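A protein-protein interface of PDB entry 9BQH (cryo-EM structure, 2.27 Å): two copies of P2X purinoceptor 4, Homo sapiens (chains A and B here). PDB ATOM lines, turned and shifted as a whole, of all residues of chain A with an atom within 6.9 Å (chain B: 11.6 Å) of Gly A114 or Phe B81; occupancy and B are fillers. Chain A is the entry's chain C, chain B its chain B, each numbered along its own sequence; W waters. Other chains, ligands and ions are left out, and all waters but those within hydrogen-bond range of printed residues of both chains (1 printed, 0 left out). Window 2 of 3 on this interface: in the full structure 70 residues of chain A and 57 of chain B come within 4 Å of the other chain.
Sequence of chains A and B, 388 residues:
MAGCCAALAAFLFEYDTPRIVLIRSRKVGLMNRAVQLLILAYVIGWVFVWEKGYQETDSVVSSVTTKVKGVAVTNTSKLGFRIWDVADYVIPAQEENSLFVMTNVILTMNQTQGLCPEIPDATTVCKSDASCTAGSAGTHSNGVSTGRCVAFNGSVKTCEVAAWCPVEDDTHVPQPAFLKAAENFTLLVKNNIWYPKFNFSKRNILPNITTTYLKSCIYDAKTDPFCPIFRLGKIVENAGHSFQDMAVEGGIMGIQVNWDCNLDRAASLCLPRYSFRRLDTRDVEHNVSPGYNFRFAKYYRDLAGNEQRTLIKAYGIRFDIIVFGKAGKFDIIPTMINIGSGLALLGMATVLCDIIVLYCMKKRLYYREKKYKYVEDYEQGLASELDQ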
ATOM      1  N   THR A 112       0.967 -29.158  19.358  1.00  0.00           N
ATOM      2  CA  THR A 112      -0.475 -28.980  19.325  1.00  0.00           C
ATOM      3  C   THR A 112      -1.008 -29.061  20.746  1.00  0.00           C
ATOM      4  O   THR A 112      -0.391 -29.670  21.620  1.00  0.00           O
ATOM      5  CB  THR A 112      -1.168 -30.032  18.448  1.00  0.00           C
ATOM      6  OG1 THR A 112      -1.049 -31.324  19.054  1.00  0.00           O
ATOM      7  CG2 THR A 112      -0.557 -30.066  17.060  1.00  0.00           C
ATOM      8  N   GLN A 113      -2.155 -28.428  20.971  1.00  0.00           N
ATOM      9  CA  GLN A 113      -2.782 -28.440  22.284  1.00  0.00           C
ATOM     10  C   GLN A 113      -3.462 -29.781  22.524  1.00  0.00           C
ATOM     11  O   GLN A 113      -4.298 -30.214  21.727  1.00  0.00           O
ATOM     12  CB  GLN A 113      -3.791 -27.299  22.395  1.00  0.00           C
ATOM     13  CG  GLN A 113      -3.145 -25.936  22.532  1.00  0.00           C
ATOM     14  CD  GLN A 113      -3.991 -24.816  21.966  1.00  0.00           C
ATOM     15  OE1 GLN A 113      -4.310 -23.857  22.661  1.00  0.00           O
ATOM     16  NE2 GLN A 113      -4.346 -24.923  20.695  1.00  0.00           N
ATOM     17  N   GLY A 114      -3.103 -30.438  23.623  1.00  0.00           N
ATOM     18  CA  GLY A 114      -3.648 -31.743  23.935  1.00  0.00           C
ATOM     19  C   GLY A 114      -3.061 -32.347  25.193  1.00  0.00           C
ATOM     20  O   GLY A 114      -2.648 -31.622  26.101  1.00  0.00           O
ATOM     21  N   LEU A 115      -3.021 -33.674  25.257  1.00  0.00           N
ATOM     22  CA  LEU A 115      -2.496 -34.408  26.401  1.00  0.00           C
ATOM     23  C   LEU A 115      -1.276 -35.207  25.969  1.00  0.00           C
ATOM     24  O   LEU A 115      -1.266 -35.801  24.888  1.00  0.00           O
ATOM     25  CB  LEU A 115      -3.554 -35.351  26.984  1.00  0.00           C
ATOM     26  CG  LEU A 115      -4.934 -34.763  27.288  1.00  0.00           C
ATOM     27  CD1 LEU A 115      -5.842 -35.842  27.836  1.00  0.00           C
ATOM     28  CD2 LEU A 115      -4.845 -33.605  28.262  1.00  0.00           C
ATOM     29  N   CYS A 116      -0.246 -35.221  26.812  1.00  0.00           N
ATOM     30  CA  CYS A 116       1.006 -35.886  26.480  1.00  0.00           C
ATOM     31  C   CYS A 116       1.734 -36.225  27.770  1.00  0.00           C
ATOM     32  O   CYS A 116       1.454 -35.635  28.818  1.00  0.00           O
ATOM     33  CB  CYS A 116       1.891 -35.000  25.589  1.00  0.00           C
ATOM     34  SG  CYS A 116       1.914 -33.259  26.062  1.00  0.00           S
ATOM     35  N   THR A 146      -3.045 -34.180  34.745  1.00  0.00           N
ATOM     36  CA  THR A 146      -4.393 -34.724  34.654  1.00  0.00           C
ATOM     37  C   THR A 146      -4.668 -35.809  35.689  1.00  0.00           C
ATOM     38  O   THR A 146      -5.811 -36.263  35.798  1.00  0.00           O
ATOM     39  CB  THR A 146      -4.644 -35.290  33.253  1.00  0.00           C
ATOM     40  OG1 THR A 146      -3.972 -36.547  33.111  1.00  0.00           O
ATOM     41  CG2 THR A 146      -4.158 -34.329  32.184  1.00  0.00           C
ATOM     42  N   GLU A 160       0.865 -37.707  32.890  1.00  0.00           N
ATOM     43  CA  GLU A 160       0.279 -37.009  31.756  1.00  0.00           C
ATOM     44  C   GLU A 160      -0.083 -35.581  32.141  1.00  0.00           C
ATOM     45  O   GLU A 160      -0.528 -35.319  33.260  1.00  0.00           O
ATOM     46  CB  GLU A 160      -0.963 -37.751  31.265  1.00  0.00           C
ATOM     47  CG  GLU A 160      -1.658 -37.095  30.089  1.00  0.00           C
ATOM     48  CD  GLU A 160      -2.861 -37.878  29.620  1.00  0.00           C
ATOM     49  OE1 GLU A 160      -3.803 -38.052  30.416  1.00  0.00           O
ATOM     50  OE2 GLU A 160      -2.863 -38.322  28.456  1.00  0.00           O
ATOM     51  N   VAL A 161       0.113 -34.653  31.204  1.00  0.00           N
ATOM     52  CA  VAL A 161      -0.182 -33.246  31.425  1.00  0.00           C
ATOM     53  C   VAL A 161      -0.991 -32.715  30.251  1.00  0.00           C
ATOM     54  O   VAL A 161      -0.943 -33.239  29.138  1.00  0.00           O
ATOM     55  CB  VAL A 161       1.096 -32.398  31.612  1.00  0.00           C
ATOM     56  CG1 VAL A 161       1.793 -32.769  32.906  1.00  0.00           C
ATOM     57  CG2 VAL A 161       2.036 -32.568  30.425  1.00  0.00           C
ATOM     58  N   ALA A 162      -1.751 -31.659  30.523  1.00  0.00           N
ATOM     59  CA  ALA A 162      -2.422 -30.877  29.492  1.00  0.00           C
ATOM     60  C   ALA A 162      -1.500 -29.722  29.128  1.00  0.00           C
ATOM     61  O   ALA A 162      -1.264 -28.829  29.947  1.00  0.00           O
ATOM     62  CB  ALA A 162      -3.779 -30.374  29.977  1.00  0.00           C
ATOM     63  N   ALA A 163      -0.972 -29.742  27.911  1.00  0.00           N
ATOM     64  CA  ALA A 163      -0.004 -28.744  27.482  1.00  0.00           C
ATOM     65  C   ALA A 163       0.012 -28.711  25.962  1.00  0.00           C
ATOM     66  O   ALA A 163      -0.742 -29.422  25.297  1.00  0.00           O
ATOM     67  CB  ALA A 163       1.386 -29.052  28.040  1.00  0.00           C
ATOM     68  N   TRP A 164       0.874 -27.859  25.416  1.00  0.00           N
ATOM     69  CA  TRP A 164       1.269 -27.982  24.022  1.00  0.00           C
ATOM     70  C   TRP A 164       2.181 -29.195  23.888  1.00  0.00           C
ATOM     71  O   TRP A 164       3.175 -29.312  24.609  1.00  0.00           O
ATOM     72  CB  TRP A 164       1.984 -26.717  23.560  1.00  0.00           C
ATOM     73  CG  TRP A 164       1.114 -25.510  23.400  1.00  0.00           C
ATOM     74  CD1 TRP A 164       0.791 -24.603  24.361  1.00  0.00           C
ATOM     75  CD2 TRP A 164       0.478 -25.062  22.198  1.00  0.00           C
ATOM     76  NE1 TRP A 164      -0.007 -23.622  23.839  1.00  0.00           N
ATOM     77  CE2 TRP A 164      -0.216 -23.880  22.511  1.00  0.00           C
ATOM     78  CE3 TRP A 164       0.430 -25.546  20.889  1.00  0.00           C
ATOM     79  CZ2 TRP A 164      -0.952 -23.176  21.564  1.00  0.00           C
ATOM     80  CZ3 TRP A 164      -0.303 -24.848  19.951  1.00  0.00           C
ATOM     81  CH2 TRP A 164      -0.983 -23.676  20.291  1.00  0.00           C
ATOM     82  N   CYS A 165       1.845 -30.101  22.973  1.00  0.00           N
ATOM     83  CA  CYS A 165       2.482 -31.402  22.923  1.00  0.00           C
ATOM     84  C   CYS A 165       3.151 -31.633  21.575  1.00  0.00           C
ATOM     85  O   CYS A 165       2.601 -31.244  20.542  1.00  0.00           O
ATOM     86  CB  CYS A 165       1.451 -32.511  23.172  1.00  0.00           C
ATOM     87  SG  CYS A 165       0.620 -32.383  24.763  1.00  0.00           S
ATOM     88  N   VAL B  71       0.548 -21.893  34.075  1.00  0.00           N
ATOM     89  CA  VAL B  71      -0.182 -22.297  32.881  1.00  0.00           C
ATOM     90  C   VAL B  71      -1.658 -22.390  33.238  1.00  0.00           C
ATOM     91  O   VAL B  71      -2.016 -22.820  34.337  1.00  0.00           O
ATOM     92  CB  VAL B  71       0.352 -23.634  32.318  1.00  0.00           C
ATOM     93  CG1 VAL B  71       0.325 -24.714  33.379  1.00  0.00           C
ATOM     94  CG2 VAL B  71      -0.441 -24.068  31.098  1.00  0.00           C
ATOM     95  N   ALA B  72      -2.514 -21.964  32.314  1.00  0.00           N
ATOM     96  CA  ALA B  72      -3.959 -22.019  32.480  1.00  0.00           C
ATOM     97  C   ALA B  72      -4.562 -22.897  31.397  1.00  0.00           C
ATOM     98  O   ALA B  72      -4.120 -22.870  30.246  1.00  0.00           O
ATOM     99  CB  ALA B  72      -4.578 -20.622  32.424  1.00  0.00           C
ATOM    100  N   VAL B  73      -5.568 -23.684  31.770  1.00  0.00           N
ATOM    101  CA  VAL B  73      -6.276 -24.557  30.844  1.00  0.00           C
ATOM    102  C   VAL B  73      -7.750 -24.184  30.859  1.00  0.00           C
ATOM    103  O   VAL B  73      -8.414 -24.293  31.895  1.00  0.00           O
ATOM    104  CB  VAL B  73      -6.088 -26.043  31.206  1.00  0.00           C
ATOM    105  CG1 VAL B  73      -6.772 -26.932  30.181  1.00  0.00           C
ATOM    106  CG2 VAL B  73      -4.613 -26.384  31.298  1.00  0.00           C
ATOM    107  N   THR B  74      -8.256 -23.749  29.711  1.00  0.00           N
ATOM    108  CA  THR B  74      -9.673 -23.504  29.499  1.00  0.00           C
ATOM    109  C   THR B  74     -10.158 -24.442  28.406  1.00  0.00           C
ATOM    110  O   THR B  74      -9.401 -24.791  27.498  1.00  0.00           O
ATOM    111  CB  THR B  74      -9.945 -22.048  29.088  1.00  0.00           C
ATOM    112  OG1 THR B  74      -9.541 -21.849  27.729  1.00  0.00           O
ATOM    113  CG2 THR B  74      -9.184 -21.080  29.977  1.00  0.00           C
ATOM    114  N   ASN B  75     -11.415 -24.875  28.493  1.00  0.00           N
ATOM    115  CA  ASN B  75     -11.937 -25.727  27.429  1.00  0.00           C
ATOM    116  C   ASN B  75     -13.438 -25.464  27.348  1.00  0.00           C
ATOM    117  O   ASN B  75     -14.216 -26.033  28.117  1.00  0.00           O
ATOM    118  CB  ASN B  75     -11.586 -27.184  27.699  1.00  0.00           C
ATOM    119  CG  ASN B  75     -12.465 -28.184  26.965  1.00  0.00           C
ATOM    120  OD1 ASN B  75     -12.368 -28.297  25.746  1.00  0.00           O
ATOM    121  ND2 ASN B  75     -13.243 -28.975  27.686  1.00  0.00           N
ATOM    122  N   THR B  76     -13.821 -24.583  26.428  1.00  0.00           N
ATOM    123  CA  THR B  76     -15.184 -24.109  26.243  1.00  0.00           C
ATOM    124  C   THR B  76     -15.677 -24.501  24.853  1.00  0.00           C
ATOM    125  O   THR B  76     -15.017 -25.236  24.117  1.00  0.00           O
ATOM    126  CB  THR B  76     -15.270 -22.590  26.432  1.00  0.00           C
ATOM    127  OG1 THR B  76     -14.725 -21.931  25.281  1.00  0.00           O
ATOM    128  CG2 THR B  76     -14.510 -22.149  27.674  1.00  0.00           C
ATOM    129  N   SER B  77     -16.857 -23.992  24.495  1.00  0.00           N
ATOM    130  CA  SER B  77     -17.506 -24.361  23.242  1.00  0.00           C
ATOM    131  C   SER B  77     -16.993 -23.546  22.056  1.00  0.00           C
ATOM    132  O   SER B  77     -16.662 -24.113  21.011  1.00  0.00           O
ATOM    133  CB  SER B  77     -19.022 -24.189  23.373  1.00  0.00           C
ATOM    134  OG  SER B  77     -19.555 -25.092  24.326  1.00  0.00           O
ATOM    135  N   LYS B  78     -16.926 -22.222  22.200  1.00  0.00           N
ATOM    136  CA  LYS B  78     -16.524 -21.378  21.080  1.00  0.00           C
ATOM    137  C   LYS B  78     -15.093 -21.673  20.647  1.00  0.00           C
ATOM    138  O   LYS B  78     -14.821 -21.869  19.457  1.00  0.00           O
ATOM    139  CB  LYS B  78     -16.677 -19.905  21.457  1.00  0.00           C
ATOM    140  N   LEU B  79     -14.162 -21.714  21.601  1.00  0.00           N
ATOM    141  CA  LEU B  79     -12.751 -21.902  21.296  1.00  0.00           C
ATOM    142  C   LEU B  79     -12.286 -23.344  21.429  1.00  0.00           C
ATOM    143  O   LEU B  79     -11.248 -23.694  20.859  1.00  0.00           O
ATOM    144  CB  LEU B  79     -11.889 -21.022  22.208  1.00  0.00           C
ATOM    145  CG  LEU B  79     -12.130 -19.514  22.130  1.00  0.00           C
ATOM    146  CD1 LEU B  79     -11.254 -18.788  23.132  1.00  0.00           C
ATOM    147  CD2 LEU B  79     -11.872 -18.999  20.726  1.00  0.00           C
ATOM    148  N   GLY B  80     -13.019 -24.182  22.154  1.00  0.00           N
ATOM    149  CA  GLY B  80     -12.577 -25.544  22.374  1.00  0.00           C
ATOM    150  C   GLY B  80     -11.517 -25.630  23.461  1.00  0.00           C
ATOM    151  O   GLY B  80     -11.393 -24.753  24.316  1.00  0.00           O
ATOM    152  N   PHE B  81     -10.743 -26.709  23.412  1.00  0.00           N
ATOM    153  CA  PHE B  81      -9.671 -26.949  24.370  1.00  0.00           C
ATOM    154  C   PHE B  81      -8.485 -26.050  24.037  1.00  0.00           C
ATOM    155  O   PHE B  81      -7.952 -26.108  22.924  1.00  0.00           O
ATOM    156  CB  PHE B  81      -9.266 -28.422  24.327  1.00  0.00           C
ATOM    157  CG  PHE B  81      -8.257 -28.815  25.364  1.00  0.00           C
ATOM    158  CD1 PHE B  81      -8.621 -28.948  26.689  1.00  0.00           C
ATOM    159  CD2 PHE B  81      -6.941 -29.056  25.010  1.00  0.00           C
ATOM    160  CE1 PHE B  81      -7.697 -29.314  27.639  1.00  0.00           C
ATOM    161  CE2 PHE B  81      -6.015 -29.420  25.957  1.00  0.00           C
ATOM    162  CZ  PHE B  81      -6.393 -29.551  27.272  1.00  0.00           C
ATOM    163  N   ARG B  82      -8.069 -25.223  24.995  1.00  0.00           N
ATOM    164  CA  ARG B  82      -6.982 -24.279  24.789  1.00  0.00           C
ATOM    165  C   ARG B  82      -5.996 -24.352  25.943  1.00  0.00           C
ATOM    166  O   ARG B  82      -6.370 -24.608  27.089  1.00  0.00           O
ATOM    167  CB  ARG B  82      -7.498 -22.841  24.653  1.00  0.00           C
ATOM    168  CG  ARG B  82      -8.493 -22.626  23.522  1.00  0.00           C
ATOM    169  CD  ARG B  82      -7.834 -22.671  22.158  1.00  0.00           C
ATOM    170  NE  ARG B  82      -6.684 -21.777  22.071  1.00  0.00           N
ATOM    171  CZ  ARG B  82      -6.621 -20.681  21.326  1.00  0.00           C
ATOM    172  NH1 ARG B  82      -7.632 -20.293  20.568  1.00  0.00           N
ATOM    173  NH2 ARG B  82      -5.509 -19.951  21.344  1.00  0.00           N
ATOM    174  N   ILE B  83      -4.729 -24.118  25.623  1.00  0.00           N
ATOM    175  CA  ILE B  83      -3.647 -24.067  26.597  1.00  0.00           C
ATOM    176  C   ILE B  83      -3.040 -22.676  26.545  1.00  0.00           C
ATOM    177  O   ILE B  83      -2.813 -22.131  25.459  1.00  0.00           O
ATOM    178  CB  ILE B  83      -2.565 -25.138  26.328  1.00  0.00           C
ATOM    179  CG1 ILE B  83      -3.175 -26.543  26.317  1.00  0.00           C
ATOM    180  CG2 ILE B  83      -1.451 -25.039  27.360  1.00  0.00           C
ATOM    181  CD1 ILE B  83      -3.588 -27.050  27.672  1.00  0.00           C
ATOM    182  N   TRP B  84      -2.791 -22.096  27.716  1.00  0.00           N
ATOM    183  CA  TRP B  84      -2.178 -20.776  27.832  1.00  0.00           C
ATOM    184  C   TRP B  84      -0.964 -20.901  28.746  1.00  0.00           C
ATOM    185  O   TRP B  84      -1.105 -20.908  29.971  1.00  0.00           O
ATOM    186  CB  TRP B  84      -3.172 -19.749  28.367  1.00  0.00           C
ATOM    187  CG  TRP B  84      -4.494 -19.781  27.672  1.00  0.00           C
ATOM    188  CD1 TRP B  84      -5.557 -20.577  27.972  1.00  0.00           C
ATOM    189  CD2 TRP B  84      -4.894 -18.983  26.554  1.00  0.00           C
ATOM    190  NE1 TRP B  84      -6.592 -20.328  27.109  1.00  0.00           N
ATOM    191  CE2 TRP B  84      -6.210 -19.352  26.228  1.00  0.00           C
ATOM    192  CE3 TRP B  84      -4.263 -17.993  25.796  1.00  0.00           C
ATOM    193  CZ2 TRP B  84      -6.911 -18.763  25.180  1.00  0.00           C
ATOM    194  CZ3 TRP B  84      -4.960 -17.411  24.756  1.00  0.00           C
ATOM    195  CH2 TRP B  84      -6.270 -17.797  24.457  1.00  0.00           C
ATOM    196  N   ASP B  85       0.222 -21.004  28.154  1.00  0.00           N
ATOM    197  CA  ASP B  85       1.472 -20.996  28.894  1.00  0.00           C
ATOM    198  C   ASP B  85       2.175 -19.659  28.668  1.00  0.00           C
ATOM    199  O   ASP B  85       1.626 -18.741  28.055  1.00  0.00           O
ATOM    200  CB  ASP B  85       2.344 -22.195  28.506  1.00  0.00           C
ATOM    201  CG  ASP B  85       2.755 -22.190  27.049  1.00  0.00           C
ATOM    202  OD1 ASP B  85       2.718 -21.129  26.399  1.00  0.00           O
ATOM    203  OD2 ASP B  85       3.147 -23.264  26.556  1.00  0.00           O
ATOM    204  N   ASP B  88       2.069 -17.724  25.565  1.00  0.00           N
ATOM    205  CA  ASP B  88       0.751 -17.329  25.086  1.00  0.00           C
ATOM    206  C   ASP B  88       0.224 -16.059  25.740  1.00  0.00           C
ATOM    207  O   ASP B  88      -0.401 -15.241  25.060  1.00  0.00           O
ATOM    208  CB  ASP B  88      -0.255 -18.458  25.322  1.00  0.00           C
ATOM    209  CG  ASP B  88      -0.020 -19.644  24.419  1.00  0.00           C
ATOM    210  OD1 ASP B  88      -0.160 -19.494  23.190  1.00  0.00           O
ATOM    211  OD2 ASP B  88       0.303 -20.730  24.937  1.00  0.00           O
ATOM    212  N   LEU B 107     -11.450 -12.788  20.699  1.00  0.00           N
ATOM    213  CA  LEU B 107     -10.778 -13.332  19.525  1.00  0.00           C
ATOM    214  C   LEU B 107     -11.666 -13.190  18.297  1.00  0.00           C
ATOM    215  O   LEU B 107     -12.887 -13.349  18.385  1.00  0.00           O
ATOM    216  CB  LEU B 107     -10.416 -14.805  19.733  1.00  0.00           C
ATOM    217  CG  LEU B 107      -9.372 -15.125  20.808  1.00  0.00           C
ATOM    218  CD1 LEU B 107      -9.285 -16.617  21.027  1.00  0.00           C
ATOM    219  CD2 LEU B 107      -8.012 -14.575  20.432  1.00  0.00           C
ATOM    220  N   MET B 109     -11.324 -14.809  14.462  1.00  0.00           N
ATOM    221  CA  MET B 109     -10.553 -15.728  13.635  1.00  0.00           C
ATOM    222  C   MET B 109     -10.945 -15.561  12.171  1.00  0.00           C
ATOM    223  O   MET B 109     -12.072 -15.163  11.863  1.00  0.00           O
ATOM    224  CB  MET B 109     -10.773 -17.183  14.067  1.00  0.00           C
ATOM    225  CG  MET B 109     -11.194 -17.390  15.530  1.00  0.00           C
ATOM    226  SD  MET B 109      -9.829 -17.570  16.693  1.00  0.00           S
ATOM    227  CE  MET B 109      -9.011 -19.027  16.054  1.00  0.00           C
ATOM    228  N   PHE B 178     -11.433 -14.404  31.393  1.00  0.00           N
ATOM    229  CA  PHE B 178     -11.199 -15.668  30.706  1.00  0.00           C
ATOM    230  C   PHE B 178     -10.043 -16.433  31.340  1.00  0.00           C
ATOM    231  O   PHE B 178     -10.167 -17.622  31.654  1.00  0.00           O
ATOM    232  CB  PHE B 178     -10.930 -15.407  29.224  1.00  0.00           C
ATOM    233  CG  PHE B 178     -10.987 -16.638  28.374  1.00  0.00           C
ATOM    234  CD1 PHE B 178     -12.163 -17.353  28.248  1.00  0.00           C
ATOM    235  CD2 PHE B 178      -9.867 -17.079  27.696  1.00  0.00           C
ATOM    236  CE1 PHE B 178     -12.218 -18.484  27.469  1.00  0.00           C
ATOM    237  CE2 PHE B 178      -9.920 -18.208  26.915  1.00  0.00           C
ATOM    238  CZ  PHE B 178     -11.096 -18.909  26.801  1.00  0.00           C
ATOM    239  N   LEU B 179      -8.905 -15.770  31.522  1.00  0.00           N
ATOM    240  CA  LEU B 179      -7.756 -16.362  32.207  1.00  0.00           C
ATOM    241  C   LEU B 179      -7.705 -15.895  33.659  1.00  0.00           C
ATOM    242  O   LEU B 179      -6.786 -15.205  34.091  1.00  0.00           O
ATOM    243  CB  LEU B 179      -6.464 -16.019  31.472  1.00  0.00           C
ATOM    244  CG  LEU B 179      -6.466 -16.237  29.959  1.00  0.00           C
ATOM    245  CD1 LEU B 179      -5.108 -15.909  29.373  1.00  0.00           C
ATOM    246  CD2 LEU B 179      -6.863 -17.659  29.626  1.00  0.00           C
ATOM    247  N   LYS B 298      -2.227 -12.591  14.857  1.00  0.00           N
ATOM    248  CA  LYS B 298      -1.436 -13.683  14.312  1.00  0.00           C
ATOM    249  C   LYS B 298      -1.756 -13.803  12.831  1.00  0.00           C
ATOM    250  O   LYS B 298      -2.928 -13.846  12.451  1.00  0.00           O
ATOM    251  CB  LYS B 298      -1.745 -15.000  15.023  1.00  0.00           C
ATOM    252  CG  LYS B 298      -1.346 -15.038  16.480  1.00  0.00           C
ATOM    253  CD  LYS B 298      -1.837 -16.310  17.134  1.00  0.00           C
ATOM    254  CE  LYS B 298      -1.504 -16.349  18.609  1.00  0.00           C
ATOM    255  NZ  LYS B 298      -2.224 -17.451  19.293  1.00  0.00           N
HETATM  256  O   HOH W   1       2.792 -25.836  27.308  1.00  0.00           O
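Among the printed residues, merely in contact across the chains: Gly A114 with Phe B81, Ala A162 with Phe B81, Ala A162 with Ile B83, Ala A163 with Ile B83, Trp A164 with Ile B83 and Trp A164 with Asp B85.
Hydrophobic or aromatic side chains of chain B that line the printed part of chain A: Phe B81 and Ile B83.
Among the printed residues, 9 pairs touch across the chains.
Among the printed residues, no Asp or Glu carboxylate lies within 4 Å of a Lys or Arg side-chain nitrogen of the other chain.
OD2 of Asp B88 sits at hydrogen-bond distance from NE1 of Trp A164 (3.1 Å).
The backbone NH (N) of Ile B83 sits at hydrogen-bond distance from the side-chain amide oxygen (OE1) of Gln A113, at 3.0 Å.
The guanidinium group of Arg B82 is in hydrogen-bond range of the side-chain amide oxygen of Gln A113 (3.2 Å).
Water W1 lies within hydrogen-bond range of the side-chain carboxylate (OD2) of Asp B85 and the backbone NH (N) of Trp A164.
No position is printed for both chains.
Of the 9 pairs that touch across the chains among the printed residues, none has its exchanged pair printed and touching as well.
Gly A114 touches just one residue of chain B: Phe B81.
Of chain A, only Gly A114 and Ala A162 come within 4 Å of Phe B81.
Thr A112 touches none of the printed residues of chain B.
Printed residues of chain B within 4 Å of Gln A113: Arg B82 and Ile B83.
No residue of chain B comes within 4 Å of Leu A115.
No residue of chain B comes within 4 Å of Cys A116.
Ala A162 touches two residues of chain B.
Ala A163 touches one residue of chain B.
No residue of chain B comes within 4 Å of Cys A165.
Of the printed residues of chain A, Asp B85 touches Trp A164.
Of the printed residues of chain B, Trp A164 touches Ile B83, Asp B85 and Asp B88.
Met B109 touches none of the printed residues of chain A.
The nearest residue of chain A that does not touch Phe B81 is Gln A113 (4.3 Å).
The side-chain carboxylate (OD2) of Asp B88 is in hydrogen-bond range of the backbone NH (N) of Asp B85, at 3.2 Å.
The side-chain amide oxygen (OD1) of Asn B75 is in hydrogen-bond range of the backbone NH (N) of Phe B81 (3.3 Å).
The backbone carbonyl oxygen (O) of Thr B74 sits at hydrogen-bond distance from the backbone NH (N) of Arg B82 (2.9 Å).
The side-chain sulfur (SG) of Cys A116 is disulfide-bonded to the side-chain sulfur (SG) of Cys A165 (2.0 Å).
The backbone NH of Gly A114 lies within hydrogen-bond range of the backbone carbonyl oxygen of Ala A163, 3.1 Å away.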
